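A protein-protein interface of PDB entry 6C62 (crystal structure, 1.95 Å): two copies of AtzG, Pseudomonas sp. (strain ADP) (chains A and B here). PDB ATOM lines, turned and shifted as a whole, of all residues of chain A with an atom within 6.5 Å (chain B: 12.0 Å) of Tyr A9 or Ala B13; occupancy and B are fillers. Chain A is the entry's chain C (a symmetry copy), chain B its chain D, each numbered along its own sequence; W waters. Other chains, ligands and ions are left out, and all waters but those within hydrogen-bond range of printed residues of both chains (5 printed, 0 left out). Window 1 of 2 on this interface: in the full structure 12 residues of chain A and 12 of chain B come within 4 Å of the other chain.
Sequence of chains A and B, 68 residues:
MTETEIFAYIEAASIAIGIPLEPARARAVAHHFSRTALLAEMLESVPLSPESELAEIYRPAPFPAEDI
Among the printed residues, pairs that only touch across the chains: Met A1 with Ala B16 (3.0 Å), Glu A5 with Ile B15 (3.3 Å), Ala A8 with Ala B12 (3.6 Å), Tyr A9 with Ala B12 (3.7 Å), Tyr A9 with Ala B13 (3.6 Å), Ala A12 with Ala B8 (3.7 Å), Ala A12 with Tyr B9 (3.7 Å) and Ala A13 with Tyr B9 (3.7 Å).
Of chain A, only Tyr A9 (3.6 Å) comes within 4 Å of Ala B13. No residue of chain B comes within 4 Å of Ile A6. Ala A12 touches two residues of chain B. Ala A13 touches one residue of chain B. No residue of chain B comes within 4 Å of Ser A14. Of the printed residues of chain B, Glu A5 touches Ile B15 (3.3 Å). Printed residues of chain A within 4 Å of Tyr B9: Ala A12 (3.7 Å) and Ala A13 (3.7 Å). Printed residues of chain A within 4 Å of Ile B15: Glu A5 (3.3 Å). Printed residues of chain A within 4 Å of Ala B16: Met A1 (3.0 Å). Printed residues of chain B within 4 Å of Met A1: Ala B16 (3.0 Å). Ile B6 touches none of the printed residues of chain A. Phe A33 touches none of the printed residues of chain B. The nearest residue of chain B that does not touch Tyr A9 is Tyr B9 (4.04 Å). The nearest residue of chain A that does not touch Ala B13 is Ala A12 (6.0 Å).
Of the 13 printed residues of chain A, 6 touch a printed residue of chain B. Printed residues of chain A that touch a printed residue of chain B: Met A1, Glu A5, Ala A8, Tyr A9, Ala A12 and Ala A13. Hydrophobic or aromatic side chains of chain A that line the printed part of chain B: Met A1, Tyr A9, Ala A12 and Ala A13. Printed residues of chain B that touch a printed residue of chain A: Ala B8, Tyr B9, Ala B12, Ala B13, Ile B15 and Ala B16. Hydrophobic or aromatic side chains of chain B that line the printed part of chain A: Tyr B9, Ala B12, Ala B13, Ile B15 and Ala B16. Along chain B the printed residues that touch a printed residue of chain A span positions 8 to 16. Among the printed residues, 8 pairs touch across the chains. Among the printed residues, no Asp or Glu carboxylate lies within 4 Å of a Lys or Arg side-chain nitrogen of the other chain.
Ala A8 touches Ala B12, and with the chains exchanged Ala A12 touches Ala B8. Tyr A9 touches Ala B12, and with the chains exchanged Ala A12 touches Tyr B9. Tyr A9 touches Ala B13, and with the chains exchanged Ala A13 touches Tyr B9. Positions printed for both chains: 1, 4, 5, 6, 7, 8, 9, 10, 11, 12, 13, 14 and 33. Of the 8 pairs that touch across the chains among the printed residues, 6 have their exchanged pair printed and touching as well.
Water W1 lies within hydrogen-bond range of the backbone carbonyl oxygen (O) of Glu A5 (2.7 Å) and the backbone carbonyl oxygen (O) of Ala B12 (2.8 Å). Water W5 lies within hydrogen-bond range of the backbone carbonyl oxygen (O) of Ala B16 (2.8 Å), the backbone carbonyl oxygen (O) of Ile B15 (3.1 Å) and the backbone NH (N) of Met A1 (3.4 Å). Water W4 lies within hydrogen-bond range of the backbone carbonyl oxygen of Glu B5 (2.8 Å) and the backbone carbonyl oxygen of Ala A12 (2.9 Å). Water W2 lies within hydrogen-bond range of the side-chain hydroxyl of Tyr B9 (2.9 Å) and the side-chain hydroxyl of Tyr A9 (3.2 Å). Water W3 bridges the side-chain hydroxyl of Tyr A9 (3.0 Å) and the side-chain hydroxyl of Tyr B9 (3.2 Å).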
ATOM      1  N   MET A   1      17.598 -14.281   7.222  1.00  0.00           N
ATOM      2  CA  MET A   1      17.689 -15.546   6.435  1.00  0.00           C
ATOM      3  C   MET A   1      18.780 -16.453   7.002  1.00  0.00           C
ATOM      4  O   MET A   1      19.981 -16.203   6.803  1.00  0.00           O
ATOM      5  CB  MET A   1      18.022 -15.240   4.966  1.00  0.00           C
ATOM      6  CG  MET A   1      16.897 -14.776   4.069  1.00  0.00           C
ATOM      7  SD  MET A   1      17.499 -14.655   2.373  1.00  0.00           S
ATOM      8  CE  MET A   1      16.265 -13.607   1.649  1.00  0.00           C
ATOM      9  N   THR A   4      19.645 -22.580   6.520  1.00  0.00           N
ATOM     10  CA  THR A   4      18.639 -23.610   6.199  1.00  0.00           C
ATOM     11  C   THR A   4      17.445 -23.039   5.403  1.00  0.00           C
ATOM     12  O   THR A   4      16.891 -23.703   4.522  1.00  0.00           O
ATOM     13  CB  THR A   4      18.100 -24.282   7.461  1.00  0.00           C
ATOM     14  OG1 THR A   4      17.427 -25.477   7.073  1.00  0.00           O
ATOM     15  CG2 THR A   4      17.148 -23.350   8.282  1.00  0.00           C
ATOM     16  N   GLU A   5      17.087 -21.791   5.708  1.00  0.00           N
ATOM     17  CA  GLU A   5      16.022 -21.108   4.997  1.00  0.00           C
ATOM     18  C   GLU A   5      16.497 -20.797   3.569  1.00  0.00           C
ATOM     19  O   GLU A   5      15.710 -20.930   2.627  1.00  0.00           O
ATOM     20  CB  GLU A   5      15.552 -19.843   5.751  1.00  0.00           C
ATOM     21  CG  GLU A   5      14.848 -20.206   7.082  1.00  0.00           C
ATOM     22  CD  GLU A   5      14.618 -19.022   8.053  1.00  0.00           C
ATOM     23  OE1 GLU A   5      15.285 -17.961   7.971  1.00  0.00           O
ATOM     24  OE2 GLU A   5      13.737 -19.152   8.916  1.00  0.00           O
ATOM     25  N   ILE A   6      17.775 -20.414   3.427  1.00  0.00           N
ATOM     26  CA  ILE A   6      18.368 -20.126   2.105  1.00  0.00           C
ATOM     27  C   ILE A   6      18.348 -21.377   1.237  1.00  0.00           C
ATOM     28  O   ILE A   6      17.934 -21.332   0.111  1.00  0.00           O
ATOM     29  CB  ILE A   6      19.791 -19.539   2.205  1.00  0.00           C
ATOM     30  CG1 ILE A   6      19.659 -18.075   2.648  1.00  0.00           C
ATOM     31  CG2 ILE A   6      20.490 -19.565   0.857  1.00  0.00           C
ATOM     32  CD1 ILE A   6      20.914 -17.375   3.113  1.00  0.00           C
ATOM     33  N   PHE A   7      18.732 -22.502   1.801  1.00  0.00           N
ATOM     34  CA  PHE A   7      18.744 -23.730   1.058  1.00  0.00           C
ATOM     35  C   PHE A   7      17.357 -24.126   0.563  1.00  0.00           C
ATOM     36  O   PHE A   7      17.171 -24.472  -0.620  1.00  0.00           O
ATOM     37  CB  PHE A   7      19.388 -24.848   1.843  1.00  0.00           C
ATOM     38  CG  PHE A   7      19.813 -25.970   0.959  1.00  0.00           C
ATOM     39  CD1 PHE A   7      20.868 -25.782   0.028  1.00  0.00           C
ATOM     40  CD2 PHE A   7      19.096 -27.185   0.941  1.00  0.00           C
ATOM     41  CE1 PHE A   7      21.212 -26.816  -0.876  1.00  0.00           C
ATOM     42  CE2 PHE A   7      19.435 -28.209   0.039  1.00  0.00           C
ATOM     43  CZ  PHE A   7      20.501 -28.030  -0.859  1.00  0.00           C
ATOM     44  N   ALA A   8      16.359 -24.047   1.442  1.00  0.00           N
ATOM     45  CA  ALA A   8      14.978 -24.321   1.000  1.00  0.00           C
ATOM     46  C   ALA A   8      14.524 -23.360  -0.092  1.00  0.00           C
ATOM     47  O   ALA A   8      13.775 -23.750  -0.971  1.00  0.00           O
ATOM     48  CB  ALA A   8      13.952 -24.329   2.179  1.00  0.00           C
ATOM     49  N   TYR A   9      14.900 -22.097   0.024  1.00  0.00           N
ATOM     50  CA  TYR A   9      14.508 -21.087  -0.969  1.00  0.00           C
ATOM     51  C   TYR A   9      15.158 -21.334  -2.352  1.00  0.00           C
ATOM     52  O   TYR A   9      14.476 -21.290  -3.370  1.00  0.00           O
ATOM     53  CB  TYR A   9      14.850 -19.684  -0.466  1.00  0.00           C
ATOM     54  CG  TYR A   9      14.546 -18.634  -1.500  1.00  0.00           C
ATOM     55  CD1 TYR A   9      13.242 -18.289  -1.785  1.00  0.00           C
ATOM     56  CD2 TYR A   9      15.559 -18.046  -2.268  1.00  0.00           C
ATOM     57  CE1 TYR A   9      12.937 -17.346  -2.744  1.00  0.00           C
ATOM     58  CE2 TYR A   9      15.276 -17.104  -3.213  1.00  0.00           C
ATOM     59  CZ  TYR A   9      13.952 -16.757  -3.450  1.00  0.00           C
ATOM     60  OH  TYR A   9      13.630 -15.810  -4.422  1.00  0.00           O
ATOM     61  N   ILE A  10      16.444 -21.592  -2.365  1.00  0.00           N
ATOM     62  CA  ILE A  10      17.187 -21.870  -3.591  1.00  0.00           C
ATOM     63  C   ILE A  10      16.546 -23.058  -4.315  1.00  0.00           C
ATOM     64  O   ILE A  10      16.293 -23.007  -5.552  1.00  0.00           O
ATOM     65  CB  ILE A  10      18.703 -22.195  -3.301  1.00  0.00           C
ATOM     66  CG1 ILE A  10      19.491 -20.995  -2.785  1.00  0.00           C
ATOM     67  CG2 ILE A  10      19.420 -22.704  -4.544  1.00  0.00           C
ATOM     68  CD1 ILE A  10      19.215 -19.662  -3.380  1.00  0.00           C
ATOM     69  N   GLU A  11      16.256 -24.126  -3.557  1.00  0.00           N
ATOM     70  CA  GLU A  11      15.609 -25.289  -4.138  1.00  0.00           C
ATOM     71  C   GLU A  11      14.252 -24.988  -4.740  1.00  0.00           C
ATOM     72  O   GLU A  11      13.997 -25.342  -5.892  1.00  0.00           O
ATOM     73  CB  GLU A  11      15.455 -26.408  -3.107  1.00  0.00           C
ATOM     74  CG  GLU A  11      16.814 -26.997  -2.744  1.00  0.00           C
ATOM     75  CD  GLU A  11      16.703 -28.379  -2.069  1.00  0.00           C
ATOM     76  OE1 GLU A  11      15.952 -28.544  -1.048  1.00  0.00           O
ATOM     77  OE2 GLU A  11      17.385 -29.296  -2.597  1.00  0.00           O
ATOM     78  N   ALA A  12      13.388 -24.310  -3.977  1.00  0.00           N
ATOM     79  CA  ALA A  12      12.031 -24.024  -4.459  1.00  0.00           C
ATOM     80  C   ALA A  12      12.034 -22.985  -5.566  1.00  0.00           C
ATOM     81  O   ALA A  12      11.235 -23.092  -6.516  1.00  0.00           O
ATOM     82  CB  ALA A  12      11.128 -23.628  -3.297  1.00  0.00           C
ATOM     83  N   ALA A  13      12.843 -21.950  -5.424  1.00  0.00           N
ATOM     84  CA  ALA A  13      12.874 -20.867  -6.429  1.00  0.00           C
ATOM     85  C   ALA A  13      13.433 -21.341  -7.802  1.00  0.00           C
ATOM     86  O   ALA A  13      12.931 -20.956  -8.874  1.00  0.00           O
ATOM     87  CB  ALA A  13      13.663 -19.682  -5.953  1.00  0.00           C
ATOM     88  N   SER A  14      14.430 -22.208  -7.740  1.00  0.00           N
ATOM     89  CA  SER A  14      15.062 -22.747  -8.956  1.00  0.00           C
ATOM     90  C   SER A  14      14.043 -23.627  -9.680  1.00  0.00           C
ATOM     91  O   SER A  14      13.859 -23.484 -10.891  1.00  0.00           O
ATOM     92  CB  SER A  14      16.404 -23.473  -8.681  1.00  0.00           C
ATOM     93  OG  SER A  14      16.169 -24.630  -7.900  1.00  0.00           O
ATOM     94  N   PHE A  33      24.473 -16.719  -3.116  1.00  0.00           N
ATOM     95  CA  PHE A  33      23.275 -16.059  -2.699  1.00  0.00           C
ATOM     96  C   PHE A  33      23.380 -15.491  -1.290  1.00  0.00           C
ATOM     97  O   PHE A  33      22.893 -14.392  -1.032  1.00  0.00           O
ATOM     98  CB  PHE A  33      22.122 -17.002  -2.757  1.00  0.00           C
ATOM     99  CG  PHE A  33      20.816 -16.380  -2.481  1.00  0.00           C
ATOM    100  CD1 PHE A  33      20.319 -16.321  -1.188  1.00  0.00           C
ATOM    101  CD2 PHE A  33      20.029 -15.896  -3.518  1.00  0.00           C
ATOM    102  CE1 PHE A  33      19.099 -15.747  -0.951  1.00  0.00           C
ATOM    103  CE2 PHE A  33      18.759 -15.410  -3.265  1.00  0.00           C
ATOM    104  CZ  PHE A  33      18.295 -15.327  -2.008  1.00  0.00           C
ATOM    105  N   MET B   1       4.287 -24.352 -13.480  1.00  0.00           N
ATOM    106  CA  MET B   1       4.457 -24.635 -12.048  1.00  0.00           C
ATOM    107  C   MET B   1       3.256 -25.449 -11.586  1.00  0.00           C
ATOM    108  O   MET B   1       2.137 -24.926 -11.588  1.00  0.00           O
ATOM    109  CB  MET B   1       4.475 -23.316 -11.251  1.00  0.00           C
ATOM    110  CG  MET B   1       5.572 -22.283 -11.577  1.00  0.00           C
ATOM    111  SD  MET B   1       5.780 -21.018 -10.256  1.00  0.00           S
ATOM    112  CE  MET B   1       6.237 -22.072  -8.829  1.00  0.00           C
ATOM    113  N   THR B   4       2.028 -28.318  -6.290  1.00  0.00           N
ATOM    114  CA  THR B   4       3.019 -28.704  -5.281  1.00  0.00           C
ATOM    115  C   THR B   4       4.270 -27.808  -5.286  1.00  0.00           C
ATOM    116  O   THR B   4       4.834 -27.503  -4.241  1.00  0.00           O
ATOM    117  CB  THR B   4       3.466 -30.162  -5.462  1.00  0.00           C
ATOM    118  OG1 THR B   4       2.335 -31.028  -5.335  1.00  0.00           O
ATOM    119  CG2 THR B   4       4.523 -30.561  -4.389  1.00  0.00           C
ATOM    120  N   GLU B   5       4.681 -27.408  -6.488  1.00  0.00           N
ATOM    121  CA  GLU B   5       5.863 -26.526  -6.644  1.00  0.00           C
ATOM    122  C   GLU B   5       5.524 -25.146  -6.130  1.00  0.00           C
ATOM    123  O   GLU B   5       6.379 -24.525  -5.484  1.00  0.00           O
ATOM    124  CB  GLU B   5       6.342 -26.465  -8.131  1.00  0.00           C
ATOM    125  CG  GLU B   5       6.967 -27.835  -8.523  1.00  0.00           C
ATOM    126  CD  GLU B   5       7.192 -28.028 -10.047  1.00  0.00           C
ATOM    127  OE1 GLU B   5       6.588 -27.326 -10.868  1.00  0.00           O
ATOM    128  OE2 GLU B   5       7.993 -28.904 -10.381  1.00  0.00           O
ATOM    129  N   ILE B   6       4.272 -24.705  -6.381  1.00  0.00           N
ATOM    130  CA  ILE B   6       3.825 -23.389  -5.924  1.00  0.00           C
ATOM    131  C   ILE B   6       3.794 -23.367  -4.397  1.00  0.00           C
ATOM    132  O   ILE B   6       4.332 -22.437  -3.789  1.00  0.00           O
ATOM    133  CB  ILE B   6       2.481 -22.982  -6.523  1.00  0.00           C
ATOM    134  CG1 ILE B   6       2.725 -22.575  -7.995  1.00  0.00           C
ATOM    135  CG2 ILE B   6       1.928 -21.759  -5.764  1.00  0.00           C
ATOM    136  CD1 ILE B   6       1.450 -22.210  -8.793  1.00  0.00           C
ATOM    137  N   PHE B   7       3.248 -24.402  -3.789  1.00  0.00           N
ATOM    138  CA  PHE B   7       3.197 -24.506  -2.300  1.00  0.00           C
ATOM    139  C   PHE B   7       4.597 -24.385  -1.725  1.00  0.00           C
ATOM    140  O   PHE B   7       4.811 -23.573  -0.805  1.00  0.00           O
ATOM    141  CB  PHE B   7       2.540 -25.832  -1.835  1.00  0.00           C
ATOM    142  CG  PHE B   7       2.426 -25.997  -0.322  1.00  0.00           C
ATOM    143  CD1 PHE B   7       3.537 -26.485   0.437  1.00  0.00           C
ATOM    144  CD2 PHE B   7       1.255 -25.666   0.343  1.00  0.00           C
ATOM    145  CE1 PHE B   7       3.442 -26.635   1.835  1.00  0.00           C
ATOM    146  CE2 PHE B   7       1.154 -25.806   1.755  1.00  0.00           C
ATOM    147  CZ  PHE B   7       2.246 -26.288   2.499  1.00  0.00           C
ATOM    148  N   ALA B   8       5.546 -25.209  -2.238  1.00  0.00           N
ATOM    149  CA  ALA B   8       6.904 -25.128  -1.695  1.00  0.00           C
ATOM    150  C   ALA B   8       7.523 -23.750  -1.889  1.00  0.00           C
ATOM    151  O   ALA B   8       8.278 -23.292  -1.012  1.00  0.00           O
ATOM    152  CB  ALA B   8       7.827 -26.187  -2.284  1.00  0.00           C
ATOM    153  N   TYR B   9       7.285 -23.129  -3.033  1.00  0.00           N
ATOM    154  CA  TYR B   9       7.874 -21.823  -3.308  1.00  0.00           C
ATOM    155  C   TYR B   9       7.323 -20.715  -2.391  1.00  0.00           C
ATOM    156  O   TYR B   9       8.091 -19.924  -1.795  1.00  0.00           O
ATOM    157  CB  TYR B   9       7.643 -21.419  -4.774  1.00  0.00           C
ATOM    158  CG  TYR B   9       8.216 -20.036  -5.067  1.00  0.00           C
ATOM    159  CD1 TYR B   9       9.578 -19.818  -5.092  1.00  0.00           C
ATOM    160  CD2 TYR B   9       7.377 -18.942  -5.190  1.00  0.00           C
ATOM    161  CE1 TYR B   9      10.114 -18.570  -5.356  1.00  0.00           C
ATOM    162  CE2 TYR B   9       7.872 -17.676  -5.414  1.00  0.00           C
ATOM    163  CZ  TYR B   9       9.254 -17.488  -5.503  1.00  0.00           C
ATOM    164  OH  TYR B   9       9.758 -16.213  -5.704  1.00  0.00           O
ATOM    165  N   ILE B  10       6.002 -20.645  -2.285  1.00  0.00           N
ATOM    166  CA  ILE B  10       5.346 -19.684  -1.413  1.00  0.00           C
ATOM    167  C   ILE B  10       5.896 -19.800   0.004  1.00  0.00           C
ATOM    168  O   ILE B  10       6.278 -18.783   0.619  1.00  0.00           O
ATOM    169  CB  ILE B  10       3.790 -19.829  -1.438  1.00  0.00           C
ATOM    170  CG1 ILE B  10       3.224 -19.425  -2.794  1.00  0.00           C
ATOM    171  CG2 ILE B  10       3.108 -19.007  -0.350  1.00  0.00           C
ATOM    172  CD1 ILE B  10       3.752 -18.135  -3.397  1.00  0.00           C
ATOM    173  N   GLU B  11       5.985 -21.024   0.500  1.00  0.00           N
ATOM    174  CA  GLU B  11       6.492 -21.244   1.836  1.00  0.00           C
ATOM    175  C   GLU B  11       7.944 -20.767   2.041  1.00  0.00           C
ATOM    176  O   GLU B  11       8.197 -20.004   2.964  1.00  0.00           O
ATOM    177  CB  GLU B  11       6.429 -22.706   2.221  1.00  0.00           C
ATOM    178  CG  GLU B  11       6.941 -22.982   3.639  1.00  0.00           C
ATOM    179  CD  GLU B  11       6.737 -24.433   4.025  1.00  0.00           C
ATOM    180  OE1 GLU B  11       5.551 -24.904   4.112  1.00  0.00           O
ATOM    181  OE2 GLU B  11       7.765 -25.125   4.189  1.00  0.00           O
ATOM    182  N   ALA B  12       8.847 -21.183   1.141  1.00  0.00           N
ATOM    183  CA  ALA B  12      10.250 -20.839   1.272  1.00  0.00           C
ATOM    184  C   ALA B  12      10.500 -19.370   0.996  1.00  0.00           C
ATOM    185  O   ALA B  12      11.333 -18.748   1.685  1.00  0.00           O
ATOM    186  CB  ALA B  12      11.106 -21.702   0.326  1.00  0.00           C
ATOM    187  N   ALA B  13       9.823 -18.814  -0.009  1.00  0.00           N
ATOM    188  CA  ALA B  13      10.039 -17.395  -0.355  1.00  0.00           C
ATOM    189  C   ALA B  13       9.526 -16.443   0.711  1.00  0.00           C
ATOM    190  O   ALA B  13      10.142 -15.442   1.006  1.00  0.00           O
ATOM    191  CB  ALA B  13       9.405 -17.080  -1.683  1.00  0.00           C
ATOM    192  N   SER B  14       8.380 -16.771   1.296  1.00  0.00           N
ATOM    193  CA  SER B  14       7.750 -15.915   2.317  1.00  0.00           C
ATOM    194  C   SER B  14       8.649 -15.913   3.569  1.00  0.00           C
ATOM    195  O   SER B  14       8.953 -14.836   4.119  1.00  0.00           O
ATOM    196  CB  SER B  14       6.296 -16.338   2.629  1.00  0.00           C
ATOM    197  OG  SER B  14       6.281 -17.632   3.208  1.00  0.00           O
ATOM    198  N   ILE B  15       9.154 -17.083   3.945  1.00  0.00           N
ATOM    199  CA  ILE B  15      10.123 -17.166   5.067  1.00  0.00           C
ATOM    200  C   ILE B  15      11.387 -16.351   4.751  1.00  0.00           C
ATOM    201  O   ILE B  15      11.793 -15.523   5.574  1.00  0.00           O
ATOM    202  CB  ILE B  15      10.492 -18.615   5.454  1.00  0.00           C
ATOM    203  CG1 ILE B  15       9.287 -19.320   6.043  1.00  0.00           C
ATOM    204  CG2 ILE B  15      11.636 -18.612   6.453  1.00  0.00           C
ATOM    205  CD1 ILE B  15       9.412 -20.851   6.145  1.00  0.00           C
ATOM    206  N   ALA B  16      11.954 -16.531   3.560  1.00  0.00           N
ATOM    207  CA  ALA B  16      13.157 -15.834   3.196  1.00  0.00           C
ATOM    208  C   ALA B  16      13.058 -14.298   3.233  1.00  0.00           C
ATOM    209  O   ALA B  16      14.022 -13.614   3.587  1.00  0.00           O
ATOM    210  CB  ALA B  16      13.618 -16.234   1.795  1.00  0.00           C
ATOM    211  N   ILE B  17      11.913 -13.755   2.802  1.00  0.00           N
ATOM    212  CA  ILE B  17      11.761 -12.307   2.723  1.00  0.00           C
ATOM    213  C   ILE B  17      11.230 -11.744   4.056  1.00  0.00           C
ATOM    214  O   ILE B  17      11.139 -10.554   4.224  1.00  0.00           O
ATOM    215  CB  ILE B  17      10.858 -11.965   1.528  1.00  0.00           C
ATOM    216  CG1 ILE B  17      11.051 -10.560   0.983  1.00  0.00           C
ATOM    217  CG2 ILE B  17       9.381 -12.063   1.856  1.00  0.00           C
ATOM    218  CD1 ILE B  17      12.425 -10.227   0.467  1.00  0.00           C
ATOM    219  N   GLY B  18      10.878 -12.598   5.010  1.00  0.00           N
ATOM    220  CA  GLY B  18      10.461 -12.137   6.362  1.00  0.00           C
ATOM    221  C   GLY B  18       8.966 -11.903   6.542  1.00  0.00           C
ATOM    222  O   GLY B  18       8.563 -11.077   7.350  1.00  0.00           O
ATOM    223  N   ILE B  19       8.112 -12.611   5.786  1.00  0.00           N
ATOM    224  CA  ILE B  19       6.648 -12.485   5.958  1.00  0.00           C
ATOM    225  C   ILE B  19       6.170 -13.939   6.178  1.00  0.00           C
ATOM    226  O   ILE B  19       5.682 -14.588   5.277  1.00  0.00           O
ATOM    227  CB  ILE B  19       5.963 -11.909   4.717  1.00  0.00           C
ATOM    228  CG1 ILE B  19       6.541 -10.556   4.332  1.00  0.00           C
ATOM    229  CG2 ILE B  19       4.442 -11.785   4.923  1.00  0.00           C
ATOM    230  CD1 ILE B  19       6.190 -10.137   2.920  1.00  0.00           C
ATOM    231  N   PRO B  20       6.370 -14.517   7.376  1.00  0.00           N
ATOM    232  CA  PRO B  20       5.874 -15.859   7.703  1.00  0.00           C
ATOM    233  C   PRO B  20       4.365 -15.950   7.555  1.00  0.00           C
ATOM    234  O   PRO B  20       3.607 -15.040   7.934  1.00  0.00           O
ATOM    235  CB  PRO B  20       6.327 -16.056   9.180  1.00  0.00           C
ATOM    236  CG  PRO B  20       6.557 -14.656   9.663  1.00  0.00           C
ATOM    237  CD  PRO B  20       7.216 -14.018   8.467  1.00  0.00           C
ATOM    238  N   LEU B  21       3.936 -17.006   6.868  1.00  0.00           N
ATOM    239  CA  LEU B  21       2.515 -17.227   6.540  1.00  0.00           C
ATOM    240  C   LEU B  21       1.932 -18.454   7.267  1.00  0.00           C
ATOM    241  O   LEU B  21       2.409 -19.551   7.099  1.00  0.00           O
ATOM    242  CB  LEU B  21       2.365 -17.402   5.034  1.00  0.00           C
ATOM    243  CG  LEU B  21       2.884 -16.212   4.143  1.00  0.00           C
ATOM    244  CD1 LEU B  21       2.777 -16.556   2.668  1.00  0.00           C
ATOM    245  CD2 LEU B  21       2.131 -14.904   4.454  1.00  0.00           C
ATOM    246  N   GLU B  22       0.868 -18.231   8.028  1.00  0.00           N
ATOM    247  CA  GLU B  22       0.021 -19.303   8.561  1.00  0.00           C
ATOM    248  C   GLU B  22      -0.630 -20.108   7.435  1.00  0.00           C
ATOM    249  O   GLU B  22      -0.758 -19.598   6.333  1.00  0.00           O
ATOM    250  CB  GLU B  22      -1.069 -18.698   9.477  1.00  0.00           C
ATOM    251  CG  GLU B  22      -0.559 -18.168  10.822  1.00  0.00           C
ATOM    252  CD  GLU B  22       0.226 -19.217  11.617  1.00  0.00           C
ATOM    253  OE1 GLU B  22      -0.294 -20.368  11.839  1.00  0.00           O
ATOM    254  OE2 GLU B  22       1.392 -18.927  12.023  1.00  0.00           O
ATOM    255  N   ARG B  25      -3.391 -18.456   5.296  1.00  0.00           N
ATOM    256  CA  ARG B  25      -2.884 -17.356   4.522  1.00  0.00           C
ATOM    257  C   ARG B  25      -1.963 -17.828   3.419  1.00  0.00           C
ATOM    258  O   ARG B  25      -2.038 -17.327   2.325  1.00  0.00           O
ATOM    259  CB  ARG B  25      -2.227 -16.285   5.395  1.00  0.00           C
ATOM    260  CG  ARG B  25      -2.033 -15.015   4.577  1.00  0.00           C
ATOM    261  CD  ARG B  25      -1.371 -13.826   5.233  1.00  0.00           C
ATOM    262  NE  ARG B  25      -2.038 -13.274   6.395  1.00  0.00           N
ATOM    263  CZ  ARG B  25      -3.216 -12.672   6.411  1.00  0.00           C
ATOM    264  NH1 ARG B  25      -3.988 -12.536   5.347  1.00  0.00           N
ATOM    265  NH2 ARG B  25      -3.628 -12.196   7.564  1.00  0.00           N
ATOM    266  N   ALA B  26      -1.155 -18.853   3.656  1.00  0.00           N
ATOM    267  CA  ALA B  26      -0.297 -19.397   2.577  1.00  0.00           C
ATOM    268  C   ALA B  26      -1.152 -19.899   1.400  1.00  0.00           C
ATOM    269  O   ALA B  26      -0.784 -19.658   0.245  1.00  0.00           O
ATOM    270  CB  ALA B  26       0.606 -20.481   3.092  1.00  0.00           C
ATOM    271  N   VAL B  29      -2.391 -16.772  -0.494  1.00  0.00           N
ATOM    272  CA  VAL B  29      -1.294 -16.225  -1.245  1.00  0.00           C
ATOM    273  C   VAL B  29      -1.023 -17.098  -2.509  1.00  0.00           C
ATOM    274  O   VAL B  29      -0.896 -16.529  -3.607  1.00  0.00           O
ATOM    275  CB  VAL B  29      -0.037 -16.029  -0.388  1.00  0.00           C
ATOM    276  CG1 VAL B  29       1.157 -15.694  -1.250  1.00  0.00           C
ATOM    277  CG2 VAL B  29      -0.291 -14.959   0.688  1.00  0.00           C
ATOM    278  N   ALA B  30      -1.013 -18.436  -2.377  1.00  0.00           N
ATOM    279  CA  ALA B  30      -0.803 -19.313  -3.509  1.00  0.00           C
ATOM    280  C   ALA B  30      -1.872 -19.235  -4.573  1.00  0.00           C
ATOM    281  O   ALA B  30      -1.541 -19.332  -5.745  1.00  0.00           O
ATOM    282  CB  ALA B  30      -0.602 -20.764  -3.071  1.00  0.00           C
ATOM    283  N   PHE B  33      -1.009 -16.062  -6.468  1.00  0.00           N
ATOM    284  CA  PHE B  33       0.230 -16.285  -7.147  1.00  0.00           C
ATOM    285  C   PHE B  33       0.046 -17.166  -8.371  1.00  0.00           C
ATOM    286  O   PHE B  33       0.649 -16.906  -9.420  1.00  0.00           O
ATOM    287  CB  PHE B  33       1.230 -16.905  -6.212  1.00  0.00           C
ATOM    288  CG  PHE B  33       2.570 -17.093  -6.797  1.00  0.00           C
ATOM    289  CD1 PHE B  33       3.549 -16.117  -6.655  1.00  0.00           C
ATOM    290  CD2 PHE B  33       2.913 -18.272  -7.433  1.00  0.00           C
ATOM    291  CE1 PHE B  33       4.787 -16.297  -7.170  1.00  0.00           C
ATOM    292  CE2 PHE B  33       4.179 -18.448  -7.976  1.00  0.00           C
ATOM    293  CZ  PHE B  33       5.117 -17.448  -7.829  1.00  0.00           C
HETATM  294  O   HOH W   1      13.103 -20.334   3.155  1.00  0.00           O
HETATM  295  O   HOH W   2      12.217 -16.418  -7.268  1.00  0.00           O
HETATM  296  O   HOH W   3      11.206 -14.158  -3.738  1.00  0.00           O
HETATM  297  O   HOH W   4       9.110 -25.020  -6.111  1.00  0.00           O
HETATM  298  O   HOH W   5      14.337 -13.846   6.362  1.00  0.00           O
